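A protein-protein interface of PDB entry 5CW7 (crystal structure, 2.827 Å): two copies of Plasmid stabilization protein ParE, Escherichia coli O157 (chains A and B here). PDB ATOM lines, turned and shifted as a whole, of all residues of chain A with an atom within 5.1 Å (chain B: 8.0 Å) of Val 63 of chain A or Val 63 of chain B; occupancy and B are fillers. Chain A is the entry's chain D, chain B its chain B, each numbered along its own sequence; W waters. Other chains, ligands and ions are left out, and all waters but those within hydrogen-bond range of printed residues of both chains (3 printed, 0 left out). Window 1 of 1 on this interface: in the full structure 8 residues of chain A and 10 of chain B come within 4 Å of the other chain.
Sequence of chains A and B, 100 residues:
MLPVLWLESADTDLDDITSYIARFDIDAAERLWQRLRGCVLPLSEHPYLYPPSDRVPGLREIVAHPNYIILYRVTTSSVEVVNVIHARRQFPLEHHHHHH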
ATOM      1  N   GLU A  61      -8.566 -25.557   8.174  1.00  0.00           N
ATOM      2  CA  GLU A  61      -8.451 -25.500   9.627  1.00  0.00           C
ATOM      3  C   GLU A  61      -6.999 -25.572  10.070  1.00  0.00           C
ATOM      4  O   GLU A  61      -6.238 -26.405   9.583  1.00  0.00           O
ATOM      5  CB  GLU A  61      -9.243 -26.599  10.319  1.00  0.00           C
ATOM      6  CG  GLU A  61     -10.538 -26.943   9.669  1.00  0.00           C
ATOM      7  CD  GLU A  61     -11.399 -27.875  10.520  1.00  0.00           C
ATOM      8  OE1 GLU A  61     -10.884 -28.462  11.488  1.00  0.00           O
ATOM      9  OE2 GLU A  61     -12.592 -28.059  10.199  1.00  0.00           O
ATOM     10  N   ILE A  62      -6.626 -24.673  10.974  1.00  0.00           N
ATOM     11  CA  ILE A  62      -5.353 -24.703  11.690  1.00  0.00           C
ATOM     12  C   ILE A  62      -5.621 -25.232  13.087  1.00  0.00           C
ATOM     13  O   ILE A  62      -6.487 -24.713  13.791  1.00  0.00           O
ATOM     14  CB  ILE A  62      -4.724 -23.305  11.786  1.00  0.00           C
ATOM     15  CG1 ILE A  62      -4.479 -22.713  10.406  1.00  0.00           C
ATOM     16  CG2 ILE A  62      -3.446 -23.400  12.512  1.00  0.00           C
ATOM     17  CD1 ILE A  62      -3.908 -21.351  10.437  1.00  0.00           C
ATOM     18  N   VAL A  63      -4.897 -26.250  13.520  1.00  0.00           N
ATOM     19  CA  VAL A  63      -4.976 -26.641  14.921  1.00  0.00           C
ATOM     20  C   VAL A  63      -3.823 -25.917  15.598  1.00  0.00           C
ATOM     21  O   VAL A  63      -2.687 -26.353  15.559  1.00  0.00           O
ATOM     22  CB  VAL A  63      -4.940 -28.140  15.121  1.00  0.00           C
ATOM     23  CG1 VAL A  63      -5.290 -28.428  16.561  1.00  0.00           C
ATOM     24  CG2 VAL A  63      -5.941 -28.786  14.223  1.00  0.00           C
ATOM     25  N   ALA A  64      -4.135 -24.762  16.187  1.00  0.00           N
ATOM     26  CA  ALA A  64      -3.112 -23.858  16.677  1.00  0.00           C
ATOM     27  C   ALA A  64      -2.605 -24.295  18.028  1.00  0.00           C
ATOM     28  O   ALA A  64      -1.447 -24.046  18.380  1.00  0.00           O
ATOM     29  CB  ALA A  64      -3.682 -22.447  16.772  1.00  0.00           C
ATOM     30  N   HIS A  65      -3.467 -24.968  18.772  1.00  0.00           N
ATOM     31  CA  HIS A  65      -3.272 -25.337  20.159  1.00  0.00           C
ATOM     32  C   HIS A  65      -4.188 -26.523  20.390  1.00  0.00           C
ATOM     33  O   HIS A  65      -5.223 -26.609  19.730  1.00  0.00           O
ATOM     34  CB  HIS A  65      -3.638 -24.159  21.074  1.00  0.00           C
ATOM     35  CG  HIS A  65      -3.584 -24.485  22.522  1.00  0.00           C
ATOM     36  ND1 HIS A  65      -2.524 -24.129  23.319  1.00  0.00           N
ATOM     37  CD2 HIS A  65      -4.440 -25.158  23.316  1.00  0.00           C
ATOM     38  CE1 HIS A  65      -2.726 -24.564  24.546  1.00  0.00           C
ATOM     39  NE2 HIS A  65      -3.885 -25.191  24.571  1.00  0.00           N
ATOM     40  N   PRO A  66      -3.843 -27.467  21.276  1.00  0.00           N
ATOM     41  CA  PRO A  66      -4.753 -28.600  21.482  1.00  0.00           C
ATOM     42  C   PRO A  66      -6.186 -28.175  21.813  1.00  0.00           C
ATOM     43  O   PRO A  66      -7.109 -28.975  21.692  1.00  0.00           O
ATOM     44  CB  PRO A  66      -4.084 -29.368  22.628  1.00  0.00           C
ATOM     45  CG  PRO A  66      -2.666 -29.100  22.444  1.00  0.00           C
ATOM     46  CD  PRO A  66      -2.560 -27.688  21.968  1.00  0.00           C
ATOM     47  N   TYR A  68      -7.561 -24.940  20.476  1.00  0.00           N
ATOM     48  CA  TYR A  68      -8.086 -23.896  19.600  1.00  0.00           C
ATOM     49  C   TYR A  68      -7.823 -24.182  18.132  1.00  0.00           C
ATOM     50  O   TYR A  68      -6.762 -24.676  17.756  1.00  0.00           O
ATOM     51  CB  TYR A  68      -7.545 -22.536  19.990  1.00  0.00           C
ATOM     52  CG  TYR A  68      -8.159 -22.139  21.295  1.00  0.00           C
ATOM     53  CD1 TYR A  68      -7.485 -22.381  22.483  1.00  0.00           C
ATOM     54  CD2 TYR A  68      -9.431 -21.591  21.362  1.00  0.00           C
ATOM     55  CE1 TYR A  68      -8.030 -22.091  23.684  1.00  0.00           C
ATOM     56  CE2 TYR A  68      -9.988 -21.277  22.583  1.00  0.00           C
ATOM     57  CZ  TYR A  68      -9.270 -21.538  23.740  1.00  0.00           C
ATOM     58  OH  TYR A  68      -9.749 -21.252  24.985  1.00  0.00           O
ATOM     59  N   ILE A  69      -8.821 -23.877  17.313  1.00  0.00           N
ATOM     60  CA  ILE A  69      -8.782 -24.084  15.874  1.00  0.00           C
ATOM     61  C   ILE A  69      -9.066 -22.755  15.208  1.00  0.00           C
ATOM     62  O   ILE A  69     -10.004 -22.057  15.606  1.00  0.00           O
ATOM     63  CB  ILE A  69      -9.808 -25.141  15.435  1.00  0.00           C
ATOM     64  CG1 ILE A  69      -9.354 -26.513  15.918  1.00  0.00           C
ATOM     65  CG2 ILE A  69     -10.015 -25.092  13.956  1.00  0.00           C
ATOM     66  CD1 ILE A  69     -10.140 -27.609  15.401  1.00  0.00           C
ATOM     67  N   ARG B  35      -3.236 -37.597   8.231  1.00  0.00           N
ATOM     68  CA  ARG B  35      -3.012 -36.227   8.683  1.00  0.00           C
ATOM     69  C   ARG B  35      -1.570 -35.995   9.115  1.00  0.00           C
ATOM     70  O   ARG B  35      -0.969 -34.976   8.758  1.00  0.00           O
ATOM     71  CB  ARG B  35      -3.951 -35.856   9.823  1.00  0.00           C
ATOM     72  CG  ARG B  35      -3.578 -34.497  10.330  1.00  0.00           C
ATOM     73  CD  ARG B  35      -4.606 -33.499  10.004  1.00  0.00           C
ATOM     74  NE  ARG B  35      -5.612 -33.522  11.049  1.00  0.00           N
ATOM     75  CZ  ARG B  35      -6.861 -33.108  10.915  1.00  0.00           C
ATOM     76  NH1 ARG B  35      -7.286 -32.636   9.750  1.00  0.00           N
ATOM     77  NH2 ARG B  35      -7.676 -33.199  11.954  1.00  0.00           N
ATOM     78  N   LEU B  36      -1.019 -36.896   9.939  1.00  0.00           N
ATOM     79  CA  LEU B  36       0.364 -36.743  10.392  1.00  0.00           C
ATOM     80  C   LEU B  36       1.322 -36.701   9.217  1.00  0.00           C
ATOM     81  O   LEU B  36       2.198 -35.832   9.131  1.00  0.00           O
ATOM     82  CB  LEU B  36       0.762 -37.878  11.330  1.00  0.00           C
ATOM     83  CG  LEU B  36      -0.117 -38.120  12.549  1.00  0.00           C
ATOM     84  CD1 LEU B  36       0.306 -39.411  13.196  1.00  0.00           C
ATOM     85  CD2 LEU B  36       0.043 -36.979  13.512  1.00  0.00           C
ATOM     86  N   CYS B  39       1.243 -33.281   7.657  1.00  0.00           N
ATOM     87  CA  CYS B  39       1.902 -32.195   8.370  1.00  0.00           C
ATOM     88  C   CYS B  39       3.409 -32.205   8.172  1.00  0.00           C
ATOM     89  O   CYS B  39       4.017 -31.136   8.121  1.00  0.00           O
ATOM     90  CB  CYS B  39       1.591 -32.242   9.855  1.00  0.00           C
ATOM     91  SG  CYS B  39      -0.120 -32.146  10.250  1.00  0.00           S
ATOM     92  N   TYR B  50       6.599 -24.474  12.019  1.00  0.00           N
ATOM     93  CA  TYR B  50       5.924 -24.598  13.293  1.00  0.00           C
ATOM     94  C   TYR B  50       6.774 -24.050  14.436  1.00  0.00           C
ATOM     95  O   TYR B  50       7.996 -23.929  14.317  1.00  0.00           O
ATOM     96  CB  TYR B  50       5.571 -26.059  13.519  1.00  0.00           C
ATOM     97  CG  TYR B  50       4.681 -26.569  12.425  1.00  0.00           C
ATOM     98  CD1 TYR B  50       3.331 -26.266  12.409  1.00  0.00           C
ATOM     99  CD2 TYR B  50       5.185 -27.336  11.392  1.00  0.00           C
ATOM    100  CE1 TYR B  50       2.498 -26.725  11.393  1.00  0.00           C
ATOM    101  CE2 TYR B  50       4.365 -27.808  10.383  1.00  0.00           C
ATOM    102  CZ  TYR B  50       3.020 -27.497  10.382  1.00  0.00           C
ATOM    103  OH  TYR B  50       2.203 -27.977   9.374  1.00  0.00           O
ATOM    104  N   PRO B  51       6.156 -23.673  15.555  1.00  0.00           N
ATOM    105  CA  PRO B  51       6.854 -22.853  16.540  1.00  0.00           C
ATOM    106  C   PRO B  51       7.838 -23.665  17.377  1.00  0.00           C
ATOM    107  O   PRO B  51       7.631 -24.868  17.609  1.00  0.00           O
ATOM    108  CB  PRO B  51       5.720 -22.288  17.407  1.00  0.00           C
ATOM    109  CG  PRO B  51       4.532 -23.121  17.116  1.00  0.00           C
ATOM    110  CD  PRO B  51       4.694 -23.669  15.770  1.00  0.00           C
ATOM    111  N   ARG B  55       8.615 -26.627  25.959  1.00  0.00           N
ATOM    112  CA  ARG B  55       8.888 -27.684  26.905  1.00  0.00           C
ATOM    113  C   ARG B  55      10.164 -28.444  26.604  1.00  0.00           C
ATOM    114  O   ARG B  55      10.793 -28.958  27.529  1.00  0.00           O
ATOM    115  CB  ARG B  55       7.729 -28.664  26.891  1.00  0.00           C
ATOM    116  CG  ARG B  55       6.477 -28.013  26.522  1.00  0.00           C
ATOM    117  CD  ARG B  55       5.357 -28.953  26.619  1.00  0.00           C
ATOM    118  NE  ARG B  55       4.473 -28.874  25.489  1.00  0.00           N
ATOM    119  CZ  ARG B  55       3.385 -29.616  25.375  1.00  0.00           C
ATOM    120  NH1 ARG B  55       3.080 -30.472  26.331  1.00  0.00           N
ATOM    121  NH2 ARG B  55       2.605 -29.502  24.310  1.00  0.00           N
ATOM    122  N   ARG B  60      10.641 -28.471  17.680  1.00  0.00           N
ATOM    123  CA  ARG B  60       9.457 -27.709  17.303  1.00  0.00           C
ATOM    124  C   ARG B  60       8.229 -28.603  17.388  1.00  0.00           C
ATOM    125  O   ARG B  60       8.312 -29.798  17.136  1.00  0.00           O
ATOM    126  CB  ARG B  60       9.590 -27.150  15.906  1.00  0.00           C
ATOM    127  CG  ARG B  60      10.819 -26.326  15.729  1.00  0.00           C
ATOM    128  CD  ARG B  60      10.948 -25.794  14.338  1.00  0.00           C
ATOM    129  NE  ARG B  60      12.090 -24.921  14.244  1.00  0.00           N
ATOM    130  CZ  ARG B  60      12.014 -23.600  14.215  1.00  0.00           C
ATOM    131  NH1 ARG B  60      10.847 -22.997  14.258  1.00  0.00           N
ATOM    132  NH2 ARG B  60      13.109 -22.873  14.159  1.00  0.00           N
ATOM    133  N   GLU B  61       7.091 -28.030  17.758  1.00  0.00           N
ATOM    134  CA  GLU B  61       5.871 -28.804  17.931  1.00  0.00           C
ATOM    135  C   GLU B  61       4.852 -28.510  16.839  1.00  0.00           C
ATOM    136  O   GLU B  61       4.539 -27.351  16.576  1.00  0.00           O
ATOM    137  CB  GLU B  61       5.258 -28.566  19.311  1.00  0.00           C
ATOM    138  CG  GLU B  61       6.255 -28.729  20.428  1.00  0.00           C
ATOM    139  CD  GLU B  61       5.628 -28.654  21.817  1.00  0.00           C
ATOM    140  OE1 GLU B  61       6.358 -28.433  22.819  1.00  0.00           O
ATOM    141  OE2 GLU B  61       4.396 -28.799  21.914  1.00  0.00           O
ATOM    142  N   ILE B  62       4.363 -29.563  16.193  1.00  0.00           N
ATOM    143  CA  ILE B  62       3.195 -29.501  15.312  1.00  0.00           C
ATOM    144  C   ILE B  62       1.993 -30.001  16.088  1.00  0.00           C
ATOM    145  O   ILE B  62       1.994 -31.140  16.561  1.00  0.00           O
ATOM    146  CB  ILE B  62       3.361 -30.370  14.056  1.00  0.00           C
ATOM    147  CG1 ILE B  62       4.635 -30.040  13.297  1.00  0.00           C
ATOM    148  CG2 ILE B  62       2.155 -30.227  13.193  1.00  0.00           C
ATOM    149  CD1 ILE B  62       4.885 -30.974  12.191  1.00  0.00           C
ATOM    150  N   VAL B  63       0.939 -29.199  16.190  1.00  0.00           N
ATOM    151  CA  VAL B  63      -0.314 -29.695  16.755  1.00  0.00           C
ATOM    152  C   VAL B  63      -1.113 -30.243  15.576  1.00  0.00           C
ATOM    153  O   VAL B  63      -1.887 -29.546  14.960  1.00  0.00           O
ATOM    154  CB  VAL B  63      -1.062 -28.621  17.530  1.00  0.00           C
ATOM    155  CG1 VAL B  63      -2.224 -29.231  18.238  1.00  0.00           C
ATOM    156  CG2 VAL B  63      -0.145 -27.967  18.514  1.00  0.00           C
ATOM    157  N   ALA B  64      -0.899 -31.519  15.241  1.00  0.00           N
ATOM    158  CA  ALA B  64      -1.451 -32.041  13.992  1.00  0.00           C
ATOM    159  C   ALA B  64      -2.954 -32.230  14.071  1.00  0.00           C
ATOM    160  O   ALA B  64      -3.647 -32.174  13.054  1.00  0.00           O
ATOM    161  CB  ALA B  64      -0.776 -33.364  13.633  1.00  0.00           C
ATOM    162  N   HIS B  65      -3.462 -32.412  15.277  1.00  0.00           N
ATOM    163  CA  HIS B  65      -4.824 -32.792  15.602  1.00  0.00           C
ATOM    164  C   HIS B  65      -5.020 -32.351  17.043  1.00  0.00           C
ATOM    165  O   HIS B  65      -4.034 -32.310  17.772  1.00  0.00           O
ATOM    166  CB  HIS B  65      -4.986 -34.314  15.437  1.00  0.00           C
ATOM    167  CG  HIS B  65      -6.319 -34.828  15.859  1.00  0.00           C
ATOM    168  ND1 HIS B  65      -7.216 -35.312  14.941  1.00  0.00           N
ATOM    169  CD2 HIS B  65      -6.858 -35.076  17.077  1.00  0.00           C
ATOM    170  CE1 HIS B  65      -8.305 -35.718  15.564  1.00  0.00           C
ATOM    171  NE2 HIS B  65      -8.115 -35.582  16.861  1.00  0.00           N
ATOM    172  N   PRO B  66      -6.228 -31.971  17.485  1.00  0.00           N
ATOM    173  CA  PRO B  66      -6.324 -31.482  18.861  1.00  0.00           C
ATOM    174  C   PRO B  66      -5.894 -32.480  19.895  1.00  0.00           C
ATOM    175  O   PRO B  66      -5.676 -32.084  21.035  1.00  0.00           O
ATOM    176  CB  PRO B  66      -7.796 -31.075  18.987  1.00  0.00           C
ATOM    177  CG  PRO B  66      -8.417 -31.319  17.707  1.00  0.00           C
ATOM    178  CD  PRO B  66      -7.377 -31.490  16.699  1.00  0.00           C
ATOM    179  N   ASN B  67      -5.731 -33.747  19.540  1.00  0.00           N
ATOM    180  CA  ASN B  67      -5.239 -34.770  20.456  1.00  0.00           C
ATOM    181  C   ASN B  67      -3.822 -35.266  20.164  1.00  0.00           C
ATOM    182  O   ASN B  67      -3.341 -36.119  20.900  1.00  0.00           O
ATOM    183  CB  ASN B  67      -6.164 -35.995  20.460  1.00  0.00           C
ATOM    184  CG  ASN B  67      -7.382 -35.837  21.349  1.00  0.00           C
ATOM    185  OD1 ASN B  67      -7.467 -34.949  22.182  1.00  0.00           O
ATOM    186  ND2 ASN B  67      -8.309 -36.746  21.201  1.00  0.00           N
ATOM    187  N   TYR B  68      -3.141 -34.801  19.115  1.00  0.00           N
ATOM    188  CA  TYR B  68      -1.817 -35.340  18.808  1.00  0.00           C
ATOM    189  C   TYR B  68      -0.833 -34.248  18.432  1.00  0.00           C
ATOM    190  O   TYR B  68      -1.191 -33.287  17.751  1.00  0.00           O
ATOM    191  CB  TYR B  68      -1.894 -36.401  17.705  1.00  0.00           C
ATOM    192  CG  TYR B  68      -2.568 -37.622  18.254  1.00  0.00           C
ATOM    193  CD1 TYR B  68      -1.877 -38.503  19.074  1.00  0.00           C
ATOM    194  CD2 TYR B  68      -3.921 -37.848  18.044  1.00  0.00           C
ATOM    195  CE1 TYR B  68      -2.500 -39.594  19.620  1.00  0.00           C
ATOM    196  CE2 TYR B  68      -4.546 -38.928  18.587  1.00  0.00           C
ATOM    197  CZ  TYR B  68      -3.831 -39.799  19.374  1.00  0.00           C
ATOM    198  OH  TYR B  68      -4.450 -40.876  19.931  1.00  0.00           O
ATOM    199  N   ILE B  69       0.410 -34.407  18.887  1.00  0.00           N
ATOM    200  CA  ILE B  69       1.491 -33.458  18.639  1.00  0.00           C
ATOM    201  C   ILE B  69       2.672 -34.196  18.012  1.00  0.00           C
ATOM    202  O   ILE B  69       3.047 -35.270  18.483  1.00  0.00           O
ATOM    203  CB  ILE B  69       1.924 -32.752  19.938  1.00  0.00           C
ATOM    204  CG1 ILE B  69       0.787 -31.903  20.478  1.00  0.00           C
ATOM    205  CG2 ILE B  69       3.139 -31.889  19.710  1.00  0.00           C
ATOM    206  CD1 ILE B  69       1.178 -31.015  21.567  1.00  0.00           C
ATOM    207  N   ILE B  70       3.254 -33.627  16.960  1.00  0.00           N
ATOM    208  CA  ILE B  70       4.508 -34.114  16.395  1.00  0.00           C
ATOM    209  C   ILE B  70       5.662 -33.241  16.882  1.00  0.00           C
ATOM    210  O   ILE B  70       5.606 -32.021  16.761  1.00  0.00           O
ATOM    211  CB  ILE B  70       4.465 -34.118  14.859  1.00  0.00           C
ATOM    212  CG1 ILE B  70       3.293 -34.933  14.330  1.00  0.00           C
ATOM    213  CG2 ILE B  70       5.770 -34.647  14.304  1.00  0.00           C
ATOM    214  CD1 ILE B  70       2.927 -34.585  12.918  1.00  0.00           C
ATOM    215  N   LEU B  71       6.718 -33.857  17.399  1.00  0.00           N
ATOM    216  CA  LEU B  71       7.950 -33.157  17.771  1.00  0.00           C
ATOM    217  C   LEU B  71       9.014 -33.412  16.711  1.00  0.00           C
ATOM    218  O   LEU B  71       9.233 -34.556  16.317  1.00  0.00           O
ATOM    219  CB  LEU B  71       8.445 -33.630  19.142  1.00  0.00           C
ATOM    220  CG  LEU B  71       7.559 -33.298  20.340  1.00  0.00           C
ATOM    221  CD1 LEU B  71       8.060 -33.927  21.556  1.00  0.00           C
ATOM    222  CD2 LEU B  71       7.647 -31.859  20.583  1.00  0.00           C
ATOM    223  N   ALA B  87      -1.636 -35.280  23.028  1.00  0.00           N
ATOM    224  CA  ALA B  87      -1.462 -33.903  23.451  1.00  0.00           C
ATOM    225  C   ALA B  87      -1.873 -33.664  24.889  1.00  0.00           C
ATOM    226  O   ALA B  87      -1.458 -32.659  25.469  1.00  0.00           O
ATOM    227  CB  ALA B  87      -2.260 -32.982  22.542  1.00  0.00           C
HETATM  228  O   HOH W   1       0.283 -26.120  14.677  1.00  0.00           O
HETATM  229  O   HOH W   2      -2.344 -27.894  12.166  1.00  0.00           O
HETATM  230  O   HOH W   3      -6.647 -29.314  10.432  1.00  0.00           O
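O of Val 63 of chain B lies close to O of Val 63 of chain A, at 3.3 Å. O of Pro 66 of chain B sits close to O of Pro 66 of chain A.
O of Asn 67 of chain B is in hydrogen-bond range of N of Ala 87 of chain B.
Among the printed residues, pairs that only touch across the chains: Val 63 of chain A with His 65 of chain B, Val 63 of chain A with Pro 66 of chain B, His 65 of chain A with Val 63 of chain B, Pro 66 of chain A with Val 63 of chain B and Pro 66 of chain A with Ala 87 of chain B.
Val 63 of chain A touches just these residues of chain B: Val 63 (3.3 Å), His 65 (3.96 Å) and Pro 66 (3.7 Å). No residue of chain B comes within 4 Å of Ala 64 of chain A. Of the printed residues of chain B, His 65 of chain A touches Val 63. Of the printed residues of chain B, Pro 66 of chain A touches Val 63, Pro 66 and Ala 87. Val 63 of chain B touches three residues of chain A. Of the printed residues of chain A, Pro 66 of chain B touches Val 63 and Pro 66. Ile 70 of chain B touches none of the printed residues of chain A.
Of the 19 printed residues of chain B, 4 touch a printed residue of chain A. Printed residues of chain A that touch a printed residue of chain B: Val 63, His 65 and Pro 66. Hydrophobic or aromatic side chains of chain A within 4 Å of the printed part of chain B: Val 63 and Pro 66. Among the printed residues, no Asp or Glu carboxylate lies within 4 Å of a Lys or Arg side-chain nitrogen of the other chain.
Val 63 of chain A touches its own counterpart, Val 63 of chain B. Val 63 of chain A touches His 65 of chain B, and with the chains exchanged His 65 of chain A touches Val 63 of chain B. Val 63 of chain A touches Pro 66 of chain B, and with the chains exchanged Pro 66 of chain A touches Val 63 of chain B. Pro 66 of chain B touches its own counterpart, Pro 66 of chain A. Positions printed for both chains: 61, 62, 63, 64, 65, 66, 68 and 69.
Water W3 lies within hydrogen-bond range of O of Glu 61 of chain A (3.1 Å) and NH1 of Arg 35 of chain B (3.5 Å). Water W1 bridges the backbone carbonyl oxygen (O) of Val 63 of chain A and the backbone NH (N) of Val 63 of chain B. Water W2 bridges the backbone carbonyl oxygen of Val 63 of chain B (3.3 Å) and the backbone NH of Val 63 of chain A (3.3 Å).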
